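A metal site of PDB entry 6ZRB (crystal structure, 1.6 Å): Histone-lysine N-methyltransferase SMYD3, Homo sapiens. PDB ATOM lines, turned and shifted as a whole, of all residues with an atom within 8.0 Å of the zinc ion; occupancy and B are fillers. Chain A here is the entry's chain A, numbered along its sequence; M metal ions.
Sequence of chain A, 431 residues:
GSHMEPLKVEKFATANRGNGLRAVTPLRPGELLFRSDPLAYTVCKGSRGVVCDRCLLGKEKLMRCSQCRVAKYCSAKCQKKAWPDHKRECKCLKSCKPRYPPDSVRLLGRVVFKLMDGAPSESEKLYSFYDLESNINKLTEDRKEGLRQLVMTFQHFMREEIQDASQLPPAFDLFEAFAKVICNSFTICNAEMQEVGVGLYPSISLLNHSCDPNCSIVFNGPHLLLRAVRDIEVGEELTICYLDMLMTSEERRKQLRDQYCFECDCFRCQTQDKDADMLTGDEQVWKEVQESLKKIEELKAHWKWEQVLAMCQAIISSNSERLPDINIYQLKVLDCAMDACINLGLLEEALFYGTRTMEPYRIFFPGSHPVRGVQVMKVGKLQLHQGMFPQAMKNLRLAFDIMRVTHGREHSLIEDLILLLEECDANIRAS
OG of Ser 75 lies close to SG of Cys 74, at 3.3 Å.
The backbone NH (N) of Leu 57 lies close to the side-chain sulfur (SG) of Cys 55.
N of Cys 78 lies within hydrogen-bond range of OG of Ser 75.
NH2 of Arg 54 sits close to SG of Cys 78, at 3.5 Å.
The side-chain sulfur (SG) of Cys 52 sits close to the backbone NH (N) of Arg 54 (3.4 Å).
The backbone carbonyl oxygen (O) of Leu 57 sits at hydrogen-bond distance from the backbone NH (N) of Cys 52, at 2.9 Å.
Within 4 Å of the zinc ion: Cys 52, Cys 55, Cys 74 and Cys 78.
Along chain A the residues within 4 Å of the zinc ion span positions 52 to 78.
The nearest printed residue that does not touch the zinc ion is Ser 75 (4.4 Å).
The zinc ion is bound by the side-chain sulfur (SG) of Cys 74 (2.3 Å), the side-chain sulfur (SG) of Cys 55 (2.3 Å), the side-chain sulfur (SG) of Cys 78 (2.3 Å) and the side-chain sulfur (SG) of Cys 52 (2.4 Å).
The zinc ion has four donor atoms within binding distance.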
ATOM      1  N   TYR A  41      17.365  25.583 -16.264  1.00  0.00           N
ATOM      2  CA  TYR A  41      16.025  25.599 -15.677  1.00  0.00           C
ATOM      3  C   TYR A  41      15.891  26.854 -14.838  1.00  0.00           C
ATOM      4  O   TYR A  41      16.898  27.440 -14.404  1.00  0.00           O
ATOM      5  CB  TYR A  41      15.763  24.361 -14.816  1.00  0.00           C
ATOM      6  CG  TYR A  41      16.495  24.317 -13.486  1.00  0.00           C
ATOM      7  CD1 TYR A  41      17.854  24.098 -13.438  1.00  0.00           C
ATOM      8  CD2 TYR A  41      15.819  24.509 -12.303  1.00  0.00           C
ATOM      9  CE1 TYR A  41      18.523  24.050 -12.223  1.00  0.00           C
ATOM     10  CE2 TYR A  41      16.478  24.445 -11.076  1.00  0.00           C
ATOM     11  CZ  TYR A  41      17.828  24.212 -11.038  1.00  0.00           C
ATOM     12  OH  TYR A  41      18.479  24.175  -9.822  1.00  0.00           O
ATOM     13  N   VAL A  51       9.398  28.939  -3.664  1.00  0.00           N
ATOM     14  CA  VAL A  51      10.301  27.755  -3.640  1.00  0.00           C
ATOM     15  C   VAL A  51      11.741  28.230  -3.881  1.00  0.00           C
ATOM     16  O   VAL A  51      11.955  29.303  -4.470  1.00  0.00           O
ATOM     17  CB  VAL A  51       9.913  26.671  -4.663  1.00  0.00           C
ATOM     18  CG1 VAL A  51       8.441  26.263  -4.547  1.00  0.00           C
ATOM     19  CG2 VAL A  51      10.259  27.074  -6.076  1.00  0.00           C
ATOM     20  N   CYS A  52      12.687  27.405  -3.469  1.00  0.00           N
ATOM     21  CA  CYS A  52      14.123  27.663  -3.673  1.00  0.00           C
ATOM     22  C   CYS A  52      14.437  27.657  -5.182  1.00  0.00           C
ATOM     23  O   CYS A  52      14.046  26.709  -5.890  1.00  0.00           O
ATOM     24  CB  CYS A  52      14.934  26.626  -2.922  1.00  0.00           C
ATOM     25  SG  CYS A  52      16.720  26.749  -3.209  1.00  0.00           S
ATOM     26  N   ASP A  53      15.093  28.700  -5.677  1.00  0.00           N
ATOM     27  CA  ASP A  53      15.546  28.763  -7.097  1.00  0.00           C
ATOM     28  C   ASP A  53      16.306  27.497  -7.509  1.00  0.00           C
ATOM     29  O   ASP A  53      16.201  27.105  -8.668  1.00  0.00           O
ATOM     30  CB  ASP A  53      16.496  29.947  -7.313  1.00  0.00           C
ATOM     31  CG  ASP A  53      15.841  31.210  -7.841  1.00  0.00           C
ATOM     32  OD1 ASP A  53      14.793  31.644  -7.286  1.00  0.00           O
ATOM     33  OD2 ASP A  53      16.382  31.761  -8.803  1.00  0.00           O
ATOM     34  N   ARG A  54      17.115  26.928  -6.617  1.00  0.00           N
ATOM     35  CA  ARG A  54      17.980  25.790  -6.954  1.00  0.00           C
ATOM     36  C   ARG A  54      17.196  24.477  -6.802  1.00  0.00           C
ATOM     37  O   ARG A  54      17.047  23.760  -7.795  1.00  0.00           O
ATOM     38  CB  ARG A  54      19.243  25.765  -6.085  1.00  0.00           C
ATOM     39  CG  ARG A  54      20.211  24.685  -6.536  1.00  0.00           C
ATOM     40  CD  ARG A  54      21.506  24.640  -5.785  1.00  0.00           C
ATOM     41  NE  ARG A  54      22.217  23.404  -6.079  1.00  0.00           N
ATOM     42  CZ  ARG A  54      22.142  22.285  -5.356  1.00  0.00           C
ATOM     43  NH1 ARG A  54      22.858  21.233  -5.738  1.00  0.00           N
ATOM     44  NH2 ARG A  54      21.377  22.204  -4.273  1.00  0.00           N
ATOM     45  N   CYS A  55      16.783  24.124  -5.592  1.00  0.00           N
ATOM     46  CA  CYS A  55      16.242  22.763  -5.335  1.00  0.00           C
ATOM     47  C   CYS A  55      14.727  22.697  -5.544  1.00  0.00           C
ATOM     48  O   CYS A  55      14.203  21.562  -5.501  1.00  0.00           O
ATOM     49  CB  CYS A  55      16.606  22.253  -3.939  1.00  0.00           C
ATOM     50  SG  CYS A  55      15.847  23.162  -2.581  1.00  0.00           S
ATOM     51  N   LEU A  56      14.049  23.833  -5.737  1.00  0.00           N
ATOM     52  CA  LEU A  56      12.587  23.932  -6.030  1.00  0.00           C
ATOM     53  C   LEU A  56      11.764  23.337  -4.872  1.00  0.00           C
ATOM     54  O   LEU A  56      10.630  22.939  -5.128  1.00  0.00           O
ATOM     55  CB  LEU A  56      12.302  23.235  -7.357  1.00  0.00           C
ATOM     56  CG  LEU A  56      13.087  23.753  -8.567  1.00  0.00           C
ATOM     57  CD1 LEU A  56      12.804  22.903  -9.798  1.00  0.00           C
ATOM     58  CD2 LEU A  56      12.774  25.217  -8.828  1.00  0.00           C
ATOM     59  N   LEU A  57      12.272  23.372  -3.649  1.00  0.00           N
ATOM     60  CA  LEU A  57      11.525  22.991  -2.414  1.00  0.00           C
ATOM     61  C   LEU A  57      10.946  24.256  -1.774  1.00  0.00           C
ATOM     62  O   LEU A  57      11.628  25.321  -1.759  1.00  0.00           O
ATOM     63  CB  LEU A  57      12.447  22.240  -1.445  1.00  0.00           C
ATOM     64  CG  LEU A  57      13.003  20.912  -1.938  1.00  0.00           C
ATOM     65  CD1 LEU A  57      13.927  20.294  -0.887  1.00  0.00           C
ATOM     66  CD2 LEU A  57      11.888  19.939  -2.316  1.00  0.00           C
ATOM     67  N   GLY A  58       9.708  24.155  -1.288  1.00  0.00           N
ATOM     68  CA  GLY A  58       9.003  25.234  -0.584  1.00  0.00           C
ATOM     69  C   GLY A  58       9.592  25.431   0.806  1.00  0.00           C
ATOM     70  O   GLY A  58      10.041  24.442   1.404  1.00  0.00           O
ATOM     71  N   LYS A  59       9.619  26.675   1.267  1.00  0.00           N
ATOM     72  CA  LYS A  59      10.164  27.051   2.597  1.00  0.00           C
ATOM     73  C   LYS A  59       9.505  28.367   3.007  1.00  0.00           C
ATOM     74  O   LYS A  59       9.402  29.261   2.136  1.00  0.00           O
ATOM     75  CB  LYS A  59      11.694  27.131   2.561  1.00  0.00           C
ATOM     76  CG  LYS A  59      12.418  25.920   3.149  1.00  0.00           C
ATOM     77  CD  LYS A  59      12.756  26.090   4.624  1.00  0.00           C
ATOM     78  CE  LYS A  59      14.247  26.190   4.902  1.00  0.00           C
ATOM     79  NZ  LYS A  59      14.790  24.918   5.427  1.00  0.00           N
ATOM     80  N   LEU A  62      12.587  32.169   2.711  1.00  0.00           N
ATOM     81  CA  LEU A  62      13.731  32.001   1.775  1.00  0.00           C
ATOM     82  C   LEU A  62      14.696  33.174   1.966  1.00  0.00           C
ATOM     83  O   LEU A  62      14.237  34.303   2.303  1.00  0.00           O
ATOM     84  CB  LEU A  62      13.210  31.972   0.342  1.00  0.00           C
ATOM     85  CG  LEU A  62      12.308  30.791  -0.011  1.00  0.00           C
ATOM     86  CD1 LEU A  62      11.803  30.941  -1.438  1.00  0.00           C
ATOM     87  CD2 LEU A  62      13.035  29.470   0.147  1.00  0.00           C
ATOM     88  N   LYS A  72      15.969  33.497  -4.923  1.00  0.00           N
ATOM     89  CA  LYS A  72      15.755  33.190  -3.489  1.00  0.00           C
ATOM     90  C   LYS A  72      16.026  31.718  -3.256  1.00  0.00           C
ATOM     91  O   LYS A  72      15.792  30.897  -4.165  1.00  0.00           O
ATOM     92  CB  LYS A  72      14.350  33.603  -3.052  1.00  0.00           C
ATOM     93  CG  LYS A  72      14.111  35.104  -3.179  1.00  0.00           C
ATOM     94  CD  LYS A  72      12.893  35.580  -2.454  1.00  0.00           C
ATOM     95  CE  LYS A  72      12.615  37.043  -2.706  1.00  0.00           C
ATOM     96  NZ  LYS A  72      11.316  37.429  -2.112  1.00  0.00           N
ATOM     97  N   TYR A  73      16.504  31.399  -2.053  1.00  0.00           N
ATOM     98  CA  TYR A  73      17.075  30.068  -1.761  1.00  0.00           C
ATOM     99  C   TYR A  73      16.616  29.596  -0.383  1.00  0.00           C
ATOM    100  O   TYR A  73      16.311  30.420   0.495  1.00  0.00           O
ATOM    101  CB  TYR A  73      18.598  30.119  -1.850  1.00  0.00           C
ATOM    102  CG  TYR A  73      19.112  30.621  -3.184  1.00  0.00           C
ATOM    103  CD1 TYR A  73      19.195  29.769  -4.272  1.00  0.00           C
ATOM    104  CD2 TYR A  73      19.472  31.952  -3.372  1.00  0.00           C
ATOM    105  CE1 TYR A  73      19.659  30.204  -5.505  1.00  0.00           C
ATOM    106  CE2 TYR A  73      19.953  32.396  -4.595  1.00  0.00           C
ATOM    107  CZ  TYR A  73      20.034  31.522  -5.671  1.00  0.00           C
ATOM    108  OH  TYR A  73      20.517  31.949  -6.891  1.00  0.00           O
ATOM    109  N   CYS A  74      16.618  28.279  -0.207  1.00  0.00           N
ATOM    110  CA  CYS A  74      16.207  27.605   1.045  1.00  0.00           C
ATOM    111  C   CYS A  74      17.338  27.647   2.073  1.00  0.00           C
ATOM    112  O   CYS A  74      17.073  27.400   3.254  1.00  0.00           O
ATOM    113  CB  CYS A  74      15.815  26.162   0.779  1.00  0.00           C
ATOM    114  SG  CYS A  74      17.188  25.091   0.304  1.00  0.00           S
ATOM    115  N   SER A  75      18.574  27.893   1.638  1.00  0.00           N
ATOM    116  CA  SER A  75      19.784  27.596   2.430  1.00  0.00           C
ATOM    117  C   SER A  75      20.987  28.290   1.823  1.00  0.00           C
ATOM    118  O   SER A  75      20.992  28.555   0.596  1.00  0.00           O
ATOM    119  CB  SER A  75      20.030  26.106   2.518  1.00  0.00           C
ATOM    120  OG  SER A  75      20.292  25.552   1.220  1.00  0.00           O
ATOM    121  N   ALA A  76      22.009  28.525   2.639  1.00  0.00           N
ATOM    122  CA  ALA A  76      23.327  28.983   2.164  1.00  0.00           C
ATOM    123  C   ALA A  76      23.906  27.979   1.158  1.00  0.00           C
ATOM    124  O   ALA A  76      24.488  28.444   0.163  1.00  0.00           O
ATOM    125  CB  ALA A  76      24.256  29.206   3.331  1.00  0.00           C
ATOM    126  N   LYS A  77      23.705  26.675   1.361  1.00  0.00           N
ATOM    127  CA  LYS A  77      24.215  25.633   0.431  1.00  0.00           C
ATOM    128  C   LYS A  77      23.588  25.887  -0.956  1.00  0.00           C
ATOM    129  O   LYS A  77      24.329  25.887  -1.925  1.00  0.00           O
ATOM    130  CB  LYS A  77      23.898  24.207   0.909  1.00  0.00           C
ATOM    131  CG  LYS A  77      24.180  23.102  -0.099  1.00  0.00           C
ATOM    132  CD  LYS A  77      23.652  21.719   0.292  1.00  0.00           C
ATOM    133  CE  LYS A  77      23.315  20.858  -0.915  1.00  0.00           C
ATOM    134  NZ  LYS A  77      22.827  19.520  -0.524  1.00  0.00           N
ATOM    135  N   CYS A  78      22.291  26.114  -1.051  1.00  0.00           N
ATOM    136  CA  CYS A  78      21.633  26.240  -2.386  1.00  0.00           C
ATOM    137  C   CYS A  78      22.054  27.574  -3.021  1.00  0.00           C
ATOM    138  O   CYS A  78      22.373  27.584  -4.228  1.00  0.00           O
ATOM    139  CB  CYS A  78      20.117  26.123  -2.271  1.00  0.00           C
ATOM    140  SG  CYS A  78      19.557  24.399  -2.303  1.00  0.00           S
ATOM    141  N   GLN A  79      22.106  28.657  -2.240  1.00  0.00           N
ATOM    142  CA  GLN A  79      22.495  29.992  -2.790  1.00  0.00           C
ATOM    143  C   GLN A  79      23.912  29.890  -3.364  1.00  0.00           C
ATOM    144  O   GLN A  79      24.160  30.373  -4.474  1.00  0.00           O
ATOM    145  CB  GLN A  79      22.377  31.074  -1.722  1.00  0.00           C
ATOM    146  CG  GLN A  79      22.741  32.445  -2.261  1.00  0.00           C
ATOM    147  CD  GLN A  79      22.389  33.591  -1.346  1.00  0.00           C
ATOM    148  OE1 GLN A  79      21.672  33.421  -0.354  1.00  0.00           O
ATOM    149  NE2 GLN A  79      22.852  34.774  -1.709  1.00  0.00           N
HETATM  150 ZN    ZN M   1      17.303  24.809  -1.959  1.00  0.00          ZN
